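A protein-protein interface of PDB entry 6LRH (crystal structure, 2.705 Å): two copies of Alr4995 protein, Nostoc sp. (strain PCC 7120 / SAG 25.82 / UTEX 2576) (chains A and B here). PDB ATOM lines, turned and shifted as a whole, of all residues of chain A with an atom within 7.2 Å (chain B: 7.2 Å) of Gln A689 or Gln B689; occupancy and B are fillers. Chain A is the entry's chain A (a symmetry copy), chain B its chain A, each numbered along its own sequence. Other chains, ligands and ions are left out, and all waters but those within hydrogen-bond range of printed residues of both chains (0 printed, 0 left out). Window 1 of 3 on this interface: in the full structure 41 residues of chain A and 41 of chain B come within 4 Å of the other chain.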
ATOM      1  N   VAL A 474      -6.007  28.326   1.358  1.00  0.00           N
ATOM      2  CA  VAL A 474      -5.216  27.325   0.655  1.00  0.00           C
ATOM      3  C   VAL A 474      -5.348  27.533  -0.852  1.00  0.00           C
ATOM      4  O   VAL A 474      -4.382  27.379  -1.583  1.00  0.00           O
ATOM      5  CB  VAL A 474      -5.640  25.892   1.058  1.00  0.00           C
ATOM      6  CG1 VAL A 474      -5.192  24.871   0.033  1.00  0.00           C
ATOM      7  CG2 VAL A 474      -5.091  25.550   2.425  1.00  0.00           C
ATOM      8  N   ALA A 478      -1.864  28.751  -2.782  1.00  0.00           N
ATOM      9  CA  ALA A 478      -1.492  27.810  -3.830  1.00  0.00           C
ATOM     10  C   ALA A 478      -1.396  28.493  -5.180  1.00  0.00           C
ATOM     11  O   ALA A 478      -0.412  28.344  -5.894  1.00  0.00           O
ATOM     12  CB  ALA A 478      -2.480  26.681  -3.892  1.00  0.00           C
ATOM     13  N   HIS A 507       5.520  16.815   3.000  1.00  0.00           N
ATOM     14  CA  HIS A 507       4.878  17.881   2.283  1.00  0.00           C
ATOM     15  C   HIS A 507       5.831  19.040   2.055  1.00  0.00           C
ATOM     16  O   HIS A 507       5.882  19.603   0.966  1.00  0.00           O
ATOM     17  CB  HIS A 507       3.648  18.319   3.040  1.00  0.00           C
ATOM     18  CG  HIS A 507       2.614  17.247   3.140  1.00  0.00           C
ATOM     19  ND1 HIS A 507       1.969  16.941   4.316  1.00  0.00           N
ATOM     20  CD2 HIS A 507       2.125  16.401   2.207  1.00  0.00           C
ATOM     21  CE1 HIS A 507       1.122  15.953   4.103  1.00  0.00           C
ATOM     22  NE2 HIS A 507       1.200  15.608   2.831  1.00  0.00           N
ATOM     23  N   ARG A 510       8.486  17.990  -0.498  1.00  0.00           N
ATOM     24  CA  ARG A 510       7.908  18.005  -1.833  1.00  0.00           C
ATOM     25  C   ARG A 510       7.834  19.403  -2.424  1.00  0.00           C
ATOM     26  O   ARG A 510       8.082  19.574  -3.600  1.00  0.00           O
ATOM     27  CB  ARG A 510       6.521  17.389  -1.825  1.00  0.00           C
ATOM     28  CG  ARG A 510       6.180  16.751  -3.133  1.00  0.00           C
ATOM     29  CD  ARG A 510       4.885  16.027  -3.059  1.00  0.00           C
ATOM     30  NE  ARG A 510       3.846  16.798  -3.708  1.00  0.00           N
ATOM     31  CZ  ARG A 510       3.178  16.393  -4.778  1.00  0.00           C
ATOM     32  NH1 ARG A 510       3.440  15.203  -5.309  1.00  0.00           N
ATOM     33  NH2 ARG A 510       2.246  17.180  -5.308  1.00  0.00           N
ATOM     34  N   PHE A 683      -2.233  22.080   7.052  1.00  0.00           N
ATOM     35  CA  PHE A 683      -2.129  23.120   6.070  1.00  0.00           C
ATOM     36  C   PHE A 683      -1.276  22.648   4.899  1.00  0.00           C
ATOM     37  O   PHE A 683      -1.694  22.729   3.752  1.00  0.00           O
ATOM     38  CB  PHE A 683      -1.541  24.375   6.710  1.00  0.00           C
ATOM     39  CG  PHE A 683      -1.408  25.526   5.768  1.00  0.00           C
ATOM     40  CD1 PHE A 683      -2.517  26.241   5.373  1.00  0.00           C
ATOM     41  CD2 PHE A 683      -0.170  25.896   5.278  1.00  0.00           C
ATOM     42  CE1 PHE A 683      -2.394  27.285   4.504  1.00  0.00           C
ATOM     43  CE2 PHE A 683      -0.046  26.945   4.415  1.00  0.00           C
ATOM     44  CZ  PHE A 683      -1.156  27.638   4.023  1.00  0.00           C
ATOM     45  N   LEU A 684      -0.088  22.133   5.188  1.00  0.00           N
ATOM     46  CA  LEU A 684       0.830  21.690   4.148  1.00  0.00           C
ATOM     47  C   LEU A 684       0.246  20.548   3.330  1.00  0.00           C
ATOM     48  O   LEU A 684       0.533  20.400   2.156  1.00  0.00           O
ATOM     49  CB  LEU A 684       2.166  21.268   4.764  1.00  0.00           C
ATOM     50  CG  LEU A 684       3.078  22.413   5.182  1.00  0.00           C
ATOM     51  CD1 LEU A 684       4.433  21.917   5.606  1.00  0.00           C
ATOM     52  CD2 LEU A 684       3.230  23.406   4.060  1.00  0.00           C
ATOM     53  N   SER A 685      -0.571  19.739   3.976  1.00  0.00           N
ATOM     54  CA  SER A 685      -1.200  18.604   3.347  1.00  0.00           C
ATOM     55  C   SER A 685      -2.172  19.059   2.275  1.00  0.00           C
ATOM     56  O   SER A 685      -2.144  18.553   1.159  1.00  0.00           O
ATOM     57  CB  SER A 685      -1.921  17.765   4.394  1.00  0.00           C
ATOM     58  OG  SER A 685      -2.222  16.479   3.908  1.00  0.00           O
ATOM     59  N   LEU A 686      -3.032  20.010   2.634  1.00  0.00           N
ATOM     60  CA  LEU A 686      -4.006  20.609   1.727  1.00  0.00           C
ATOM     61  C   LEU A 686      -3.358  21.479   0.661  1.00  0.00           C
ATOM     62  O   LEU A 686      -3.915  21.701  -0.404  1.00  0.00           O
ATOM     63  CB  LEU A 686      -5.001  21.459   2.509  1.00  0.00           C
ATOM     64  CG  LEU A 686      -5.938  20.800   3.499  1.00  0.00           C
ATOM     65  CD1 LEU A 686      -6.649  21.844   4.285  1.00  0.00           C
ATOM     66  CD2 LEU A 686      -6.923  19.973   2.768  1.00  0.00           C
ATOM     67  N   LEU A 687      -2.187  21.995   0.974  1.00  0.00           N
ATOM     68  CA  LEU A 687      -1.506  22.891   0.080  1.00  0.00           C
ATOM     69  C   LEU A 687      -0.960  22.152  -1.115  1.00  0.00           C
ATOM     70  O   LEU A 687      -1.117  22.591  -2.239  1.00  0.00           O
ATOM     71  CB  LEU A 687      -0.387  23.619   0.817  1.00  0.00           C
ATOM     72  CG  LEU A 687       0.365  24.670   0.004  1.00  0.00           C
ATOM     73  CD1 LEU A 687      -0.614  25.677  -0.579  1.00  0.00           C
ATOM     74  CD2 LEU A 687       1.407  25.343   0.869  1.00  0.00           C
ATOM     75  N   THR A 688      -0.318  21.024  -0.874  1.00  0.00           N
ATOM     76  CA  THR A 688       0.219  20.213  -1.962  1.00  0.00           C
ATOM     77  C   THR A 688      -0.890  19.560  -2.765  1.00  0.00           C
ATOM     78  O   THR A 688      -0.793  19.376  -3.963  1.00  0.00           O
ATOM     79  CB  THR A 688       1.135  19.127  -1.441  1.00  0.00           C
ATOM     80  OG1 THR A 688       0.501  18.494  -0.331  1.00  0.00           O
ATOM     81  CG2 THR A 688       2.446  19.717  -0.998  1.00  0.00           C
ATOM     82  N   GLN A 689      -1.943  19.195  -2.070  1.00  0.00           N
ATOM     83  CA  GLN A 689      -3.116  18.653  -2.687  1.00  0.00           C
ATOM     84  C   GLN A 689      -3.723  19.673  -3.639  1.00  0.00           C
ATOM     85  O   GLN A 689      -4.133  19.333  -4.743  1.00  0.00           O
ATOM     86  CB  GLN A 689      -4.083  18.253  -1.601  1.00  0.00           C
ATOM     87  CG  GLN A 689      -5.424  17.830  -2.039  1.00  0.00           C
ATOM     88  CD  GLN A 689      -6.108  17.036  -0.960  1.00  0.00           C
ATOM     89  OE1 GLN A 689      -5.448  16.324  -0.191  1.00  0.00           O
ATOM     90  NE2 GLN A 689      -7.429  17.161  -0.876  1.00  0.00           N
ATOM     91  N   GLN A 690      -3.744  20.936  -3.225  1.00  0.00           N
ATOM     92  CA  GLN A 690      -4.286  21.993  -4.062  1.00  0.00           C
ATOM     93  C   GLN A 690      -3.369  22.331  -5.228  1.00  0.00           C
ATOM     94  O   GLN A 690      -3.830  22.672  -6.316  1.00  0.00           O
ATOM     95  CB  GLN A 690      -4.553  23.235  -3.234  1.00  0.00           C
ATOM     96  CG  GLN A 690      -5.185  24.373  -4.007  1.00  0.00           C
ATOM     97  CD  GLN A 690      -6.617  24.101  -4.419  1.00  0.00           C
ATOM     98  OE1 GLN A 690      -7.204  23.090  -4.041  1.00  0.00           O
ATOM     99  NE2 GLN A 690      -7.182  25.001  -5.206  1.00  0.00           N
ATOM    100  N   LEU A 691      -2.066  22.235  -5.009  1.00  0.00           N
ATOM    101  CA  LEU A 691      -1.125  22.474  -6.087  1.00  0.00           C
ATOM    102  C   LEU A 691      -1.188  21.371  -7.121  1.00  0.00           C
ATOM    103  O   LEU A 691      -0.757  21.553  -8.239  1.00  0.00           O
ATOM    104  CB  LEU A 691       0.288  22.594  -5.553  1.00  0.00           C
ATOM    105  CG  LEU A 691       0.643  23.880  -4.824  1.00  0.00           C
ATOM    106  CD1 LEU A 691       1.876  23.656  -3.977  1.00  0.00           C
ATOM    107  CD2 LEU A 691       0.883  24.978  -5.810  1.00  0.00           C
ATOM    108  N   ASP A 692      -1.724  20.221  -6.747  1.00  0.00           N
ATOM    109  CA  ASP A 692      -1.835  19.119  -7.686  1.00  0.00           C
ATOM    110  C   ASP A 692      -3.000  19.296  -8.629  1.00  0.00           C
ATOM    111  O   ASP A 692      -2.879  19.080  -9.827  1.00  0.00           O
ATOM    112  CB  ASP A 692      -1.977  17.799  -6.954  1.00  0.00           C
ATOM    113  CG  ASP A 692      -0.659  17.269  -6.479  1.00  0.00           C
ATOM    114  OD1 ASP A 692       0.367  17.641  -7.102  1.00  0.00           O
ATOM    115  OD2 ASP A 692      -0.646  16.489  -5.496  1.00  0.00           O
ATOM    116  N   LYS A 693      -4.139  19.694  -8.090  1.00  0.00           N
ATOM    117  CA  LYS A 693      -5.308  19.818  -8.925  1.00  0.00           C
ATOM    118  C   LYS A 693      -5.252  21.084  -9.783  1.00  0.00           C
ATOM    119  O   LYS A 693      -6.111  21.284 -10.621  1.00  0.00           O
ATOM    120  CB  LYS A 693      -6.578  19.768  -8.080  1.00  0.00           C
ATOM    121  CG  LYS A 693      -7.045  21.073  -7.519  1.00  0.00           C
ATOM    122  CD  LYS A 693      -8.443  20.917  -6.922  1.00  0.00           C
ATOM    123  CE  LYS A 693      -8.505  19.819  -5.863  1.00  0.00           C
ATOM    124  NZ  LYS A 693      -9.802  19.849  -5.114  1.00  0.00           N
ATOM    125  N   LEU A 694      -4.228  21.915  -9.603  1.00  0.00           N
ATOM    126  CA  LEU A 694      -3.973  23.008 -10.540  1.00  0.00           C
ATOM    127  C   LEU A 694      -3.035  22.539 -11.662  1.00  0.00           C
ATOM    128  O   LEU A 694      -2.703  23.298 -12.556  1.00  0.00           O
ATOM    129  CB  LEU A 694      -3.378  24.228  -9.834  1.00  0.00           C
ATOM    130  CG  LEU A 694      -4.161  25.123  -8.851  1.00  0.00           C
ATOM    131  CD1 LEU A 694      -3.373  26.376  -8.532  1.00  0.00           C
ATOM    132  CD2 LEU A 694      -5.557  25.505  -9.312  1.00  0.00           C
ATOM    133  N   VAL B 474      -8.849   9.139  11.048  1.00  0.00           N
ATOM    134  CA  VAL B 474      -9.716   9.206   9.881  1.00  0.00           C
ATOM    135  C   VAL B 474      -9.677   7.875   9.135  1.00  0.00           C
ATOM    136  O   VAL B 474     -10.694   7.416   8.638  1.00  0.00           O
ATOM    137  CB  VAL B 474      -9.314  10.377   8.951  1.00  0.00           C
ATOM    138  CG1 VAL B 474      -9.861  10.188   7.552  1.00  0.00           C
ATOM    139  CG2 VAL B 474      -9.783  11.692   9.533  1.00  0.00           C
ATOM    140  N   ALA B 478     -13.238   5.716   9.181  1.00  0.00           N
ATOM    141  CA  ALA B 478     -13.709   5.458   7.826  1.00  0.00           C
ATOM    142  C   ALA B 478     -13.871   3.973   7.568  1.00  0.00           C
ATOM    143  O   ALA B 478     -14.904   3.525   7.086  1.00  0.00           O
ATOM    144  CB  ALA B 478     -12.765   6.056   6.823  1.00  0.00           C
ATOM    145  N   HIS B 507     -20.614  17.756   3.606  1.00  0.00           N
ATOM    146  CA  HIS B 507     -19.985  16.520   3.984  1.00  0.00           C
ATOM    147  C   HIS B 507     -20.913  15.672   4.836  1.00  0.00           C
ATOM    148  O   HIS B 507     -21.017  14.466   4.635  1.00  0.00           O
ATOM    149  CB  HIS B 507     -18.695  16.821   4.707  1.00  0.00           C
ATOM    150  CG  HIS B 507     -17.692  17.512   3.843  1.00  0.00           C
ATOM    151  ND1 HIS B 507     -16.982  18.613   4.261  1.00  0.00           N
ATOM    152  CD2 HIS B 507     -17.294  17.260   2.577  1.00  0.00           C
ATOM    153  CE1 HIS B 507     -16.183  19.010   3.289  1.00  0.00           C
ATOM    154  NE2 HIS B 507     -16.356  18.205   2.257  1.00  0.00           N
ATOM    155  N   ARG B 510     -23.763  14.354   2.642  1.00  0.00           N
ATOM    156  CA  ARG B 510     -23.274  13.261   1.817  1.00  0.00           C
ATOM    157  C   ARG B 510     -23.194  11.946   2.574  1.00  0.00           C
ATOM    158  O   ARG B 510     -23.512  10.912   2.021  1.00  0.00           O
ATOM    159  CB  ARG B 510     -21.911  13.592   1.239  1.00  0.00           C
ATOM    160  CG  ARG B 510     -21.677  12.922  -0.077  1.00  0.00           C
ATOM    161  CD  ARG B 510     -20.405  13.374  -0.695  1.00  0.00           C
ATOM    162  NE  ARG B 510     -19.386  12.358  -0.537  1.00  0.00           N
ATOM    163  CZ  ARG B 510     -18.804  11.726  -1.545  1.00  0.00           C
ATOM    164  NH1 ARG B 510     -19.139  12.026  -2.795  1.00  0.00           N
ATOM    165  NH2 ARG B 510     -17.883  10.799  -1.296  1.00  0.00           N
ATOM    166  N   PHE B 683     -12.442  17.566   9.725  1.00  0.00           N
ATOM    167  CA  PHE B 683     -12.577  16.159   9.973  1.00  0.00           C
ATOM    168  C   PHE B 683     -13.520  15.536   8.951  1.00  0.00           C
ATOM    169  O   PHE B 683     -13.176  14.560   8.301  1.00  0.00           O
ATOM    170  CB  PHE B 683     -13.080  15.934  11.397  1.00  0.00           C
ATOM    171  CG  PHE B 683     -13.237  14.494  11.760  1.00  0.00           C
ATOM    172  CD1 PHE B 683     -12.133  13.712  12.020  1.00  0.00           C
ATOM    173  CD2 PHE B 683     -14.491  13.921  11.842  1.00  0.00           C
ATOM    174  CE1 PHE B 683     -12.279  12.394  12.341  1.00  0.00           C
ATOM    175  CE2 PHE B 683     -14.637  12.605  12.171  1.00  0.00           C
ATOM    176  CZ  PHE B 683     -13.534  11.839  12.415  1.00  0.00           C
ATOM    177  N   LEU B 684     -14.703  16.116   8.792  1.00  0.00           N
ATOM    178  CA  LEU B 684     -15.702  15.583   7.875  1.00  0.00           C
ATOM    179  C   LEU B 684     -15.210  15.598   6.435  1.00  0.00           C
ATOM    180  O   LEU B 684     -15.578  14.760   5.633  1.00  0.00           O
ATOM    181  CB  LEU B 684     -17.007  16.373   7.995  1.00  0.00           C
ATOM    182  CG  LEU B 684     -17.851  16.048   9.219  1.00  0.00           C
ATOM    183  CD1 LEU B 684     -19.191  16.728   9.166  1.00  0.00           C
ATOM    184  CD2 LEU B 684     -18.045  14.559   9.349  1.00  0.00           C
ATOM    185  N   SER B 685     -14.379  16.575   6.123  1.00  0.00           N
ATOM    186  CA  SER B 685     -13.831  16.735   4.799  1.00  0.00           C
ATOM    187  C   SER B 685     -12.916  15.574   4.456  1.00  0.00           C
ATOM    188  O   SER B 685     -13.035  14.988   3.386  1.00  0.00           O
ATOM    189  CB  SER B 685     -13.070  18.051   4.709  1.00  0.00           C
ATOM    190  OG  SER B 685     -12.844  18.428   3.372  1.00  0.00           O
ATOM    191  N   LEU B 686     -12.004  15.259   5.373  1.00  0.00           N
ATOM    192  CA  LEU B 686     -11.073  14.144   5.244  1.00  0.00           C
ATOM    193  C   LEU B 686     -11.760  12.791   5.342  1.00  0.00           C
ATOM    194  O   LEU B 686     -11.268  11.789   4.845  1.00  0.00           O
ATOM    195  CB  LEU B 686     -10.002  14.223   6.325  1.00  0.00           C
ATOM    196  CG  LEU B 686      -9.024  15.379   6.330  1.00  0.00           C
ATOM    197  CD1 LEU B 686      -8.228  15.354   7.588  1.00  0.00           C
ATOM    198  CD2 LEU B 686      -8.116  15.262   5.168  1.00  0.00           C
ATOM    199  N   LEU B 687     -12.891  12.768   6.019  1.00  0.00           N
ATOM    200  CA  LEU B 687     -13.600  11.537   6.242  1.00  0.00           C
ATOM    201  C   LEU B 687     -14.247  11.047   4.972  1.00  0.00           C
ATOM    202  O   LEU B 687     -14.150   9.880   4.639  1.00  0.00           O
ATOM    203  CB  LEU B 687     -14.644  11.724   7.338  1.00  0.00           C
ATOM    204  CG  LEU B 687     -15.412  10.468   7.739  1.00  0.00           C
ATOM    205  CD1 LEU B 687     -14.441   9.365   8.129  1.00  0.00           C
ATOM    206  CD2 LEU B 687     -16.373  10.787   8.863  1.00  0.00           C
ATOM    207  N   THR B 688     -14.908  11.939   4.259  1.00  0.00           N
ATOM    208  CA  THR B 688     -15.542  11.577   2.996  1.00  0.00           C
ATOM    209  C   THR B 688     -14.510  11.293   1.921  1.00  0.00           C
ATOM    210  O   THR B 688     -14.692  10.451   1.062  1.00  0.00           O
ATOM    211  CB  THR B 688     -16.457  12.676   2.502  1.00  0.00           C
ATOM    212  OG1 THR B 688     -15.772  13.922   2.620  1.00  0.00           O
ATOM    213  CG2 THR B 688     -17.716  12.718   3.324  1.00  0.00           C
ATOM    214  N   GLN B 689     -13.426  12.033   1.977  1.00  0.00           N
ATOM    215  CA  GLN B 689     -12.315  11.828   1.097  1.00  0.00           C
ATOM    216  C   GLN B 689     -11.739  10.434   1.300  1.00  0.00           C
ATOM    217  O   GLN B 689     -11.414   9.745   0.342  1.00  0.00           O
ATOM    218  CB  GLN B 689     -11.292  12.904   1.365  1.00  0.00           C
ATOM    219  CG  GLN B 689      -9.998  12.764   0.677  1.00  0.00           C
ATOM    220  CD  GLN B 689      -9.270  14.081   0.645  1.00  0.00           C
ATOM    221  OE1 GLN B 689      -9.901  15.145   0.581  1.00  0.00           O
ATOM    222  NE2 GLN B 689      -7.944  14.029   0.708  1.00  0.00           N
ATOM    223  N   GLN B 690     -11.649  10.004   2.555  1.00  0.00           N
ATOM    224  CA  GLN B 690     -11.129   8.682   2.861  1.00  0.00           C
ATOM    225  C   GLN B 690     -12.109   7.578   2.493  1.00  0.00           C
ATOM    226  O   GLN B 690     -11.709   6.490   2.083  1.00  0.00           O
ATOM    227  CB  GLN B 690     -10.767   8.586   4.331  1.00  0.00           C
ATOM    228  CG  GLN B 690     -10.151   7.264   4.735  1.00  0.00           C
ATOM    229  CD  GLN B 690      -8.759   7.052   4.176  1.00  0.00           C
ATOM    230  OE1 GLN B 690      -8.181   7.943   3.558  1.00  0.00           O
ATOM    231  NE2 GLN B 690      -8.218   5.864   4.385  1.00  0.00           N
ATOM    232  N   LEU B 691     -13.397   7.853   2.633  1.00  0.00           N
ATOM    233  CA  LEU B 691     -14.399   6.880   2.240  1.00  0.00           C
ATOM    234  C   LEU B 691     -14.440   6.717   0.736  1.00  0.00           C
ATOM    235  O   LEU B 691     -14.937   5.729   0.240  1.00  0.00           O
ATOM    236  CB  LEU B 691     -15.769   7.280   2.749  1.00  0.00           C
ATOM    237  CG  LEU B 691     -16.033   7.100   4.235  1.00  0.00           C
ATOM    238  CD1 LEU B 691     -17.214   7.951   4.644  1.00  0.00           C
ATOM    239  CD2 LEU B 691     -16.301   5.660   4.536  1.00  0.00           C
ATOM    240  N   ASP B 692     -13.918   7.690   0.007  1.00  0.00           N
ATOM    241  CA  ASP B 692     -13.906   7.600  -1.442  1.00  0.00           C
ATOM    242  C   ASP B 692     -12.801   6.703  -1.942  1.00  0.00           C
ATOM    243  O   ASP B 692     -13.007   5.881  -2.824  1.00  0.00           O
ATOM    244  CB  ASP B 692     -13.759   8.974  -2.066  1.00  0.00           C
ATOM    245  CG  ASP B 692     -15.060   9.715  -2.117  1.00  0.00           C
ATOM    246  OD1 ASP B 692     -16.112   9.028  -2.127  1.00  0.00           O
ATOM    247  OD2 ASP B 692     -15.034  10.969  -2.151  1.00  0.00           O
ATOM    248  N   LYS B 693     -11.616   6.856  -1.377  1.00  0.00           N
ATOM    249  CA  LYS B 693     -10.501   6.077  -1.855  1.00  0.00           C
ATOM    250  C   LYS B 693     -10.572   4.633  -1.355  1.00  0.00           C
ATOM    251  O   LYS B 693      -9.764   3.815  -1.754  1.00  0.00           O
ATOM    252  CB  LYS B 693      -9.180   6.740  -1.472  1.00  0.00           C
ATOM    253  CG  LYS B 693      -8.635   6.387  -0.125  1.00  0.00           C
ATOM    254  CD  LYS B 693      -7.207   6.911   0.016  1.00  0.00           C
ATOM    255  CE  LYS B 693      -7.111   8.415  -0.230  1.00  0.00           C
ATOM    256  NZ  LYS B 693      -5.767   8.952   0.158  1.00  0.00           N
ATOM    257  N   LEU B 694     -11.554   4.309  -0.517  1.00  0.00           N
ATOM    258  CA  LEU B 694     -11.834   2.912  -0.190  1.00  0.00           C
ATOM    259  C   LEU B 694     -12.858   2.330  -1.175  1.00  0.00           C
ATOM    260  O   LEU B 694     -13.223   1.171  -1.082  1.00  0.00           O
ATOM    261  CB  LEU B 694     -12.341   2.761   1.246  1.00  0.00           C
ATOM    262  CG  LEU B 694     -11.466   2.981   2.497  1.00  0.00           C
ATOM    263  CD1 LEU B 694     -12.190   2.507   3.741  1.00  0.00           C
ATOM    264  CD2 LEU B 694     -10.091   2.337   2.434  1.00  0.00           C
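Gln A689 touches its own counterpart, Gln B689.
Among the printed residues, pairs that only touch across the chains: Gln A689 with Gln B689.
Printed residues of chain B that touch a printed residue of chain A: Gln B689.
Of the 16 printed residues of chain A, 1 touches a printed residue of chain B.
Among the printed residues, 1 pair touches across the chains.
Among the printed residues, no Asp or Glu carboxylate lies within 4 Å of a Lys or Arg side-chain nitrogen of the other chain.
Gln A689 touches just one residue of chain B: Gln B689.
Gln B689 touches one residue of chain A.
The nearest residue of chain A that does not touch Gln B689 is Leu A686 (6.1 Å).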
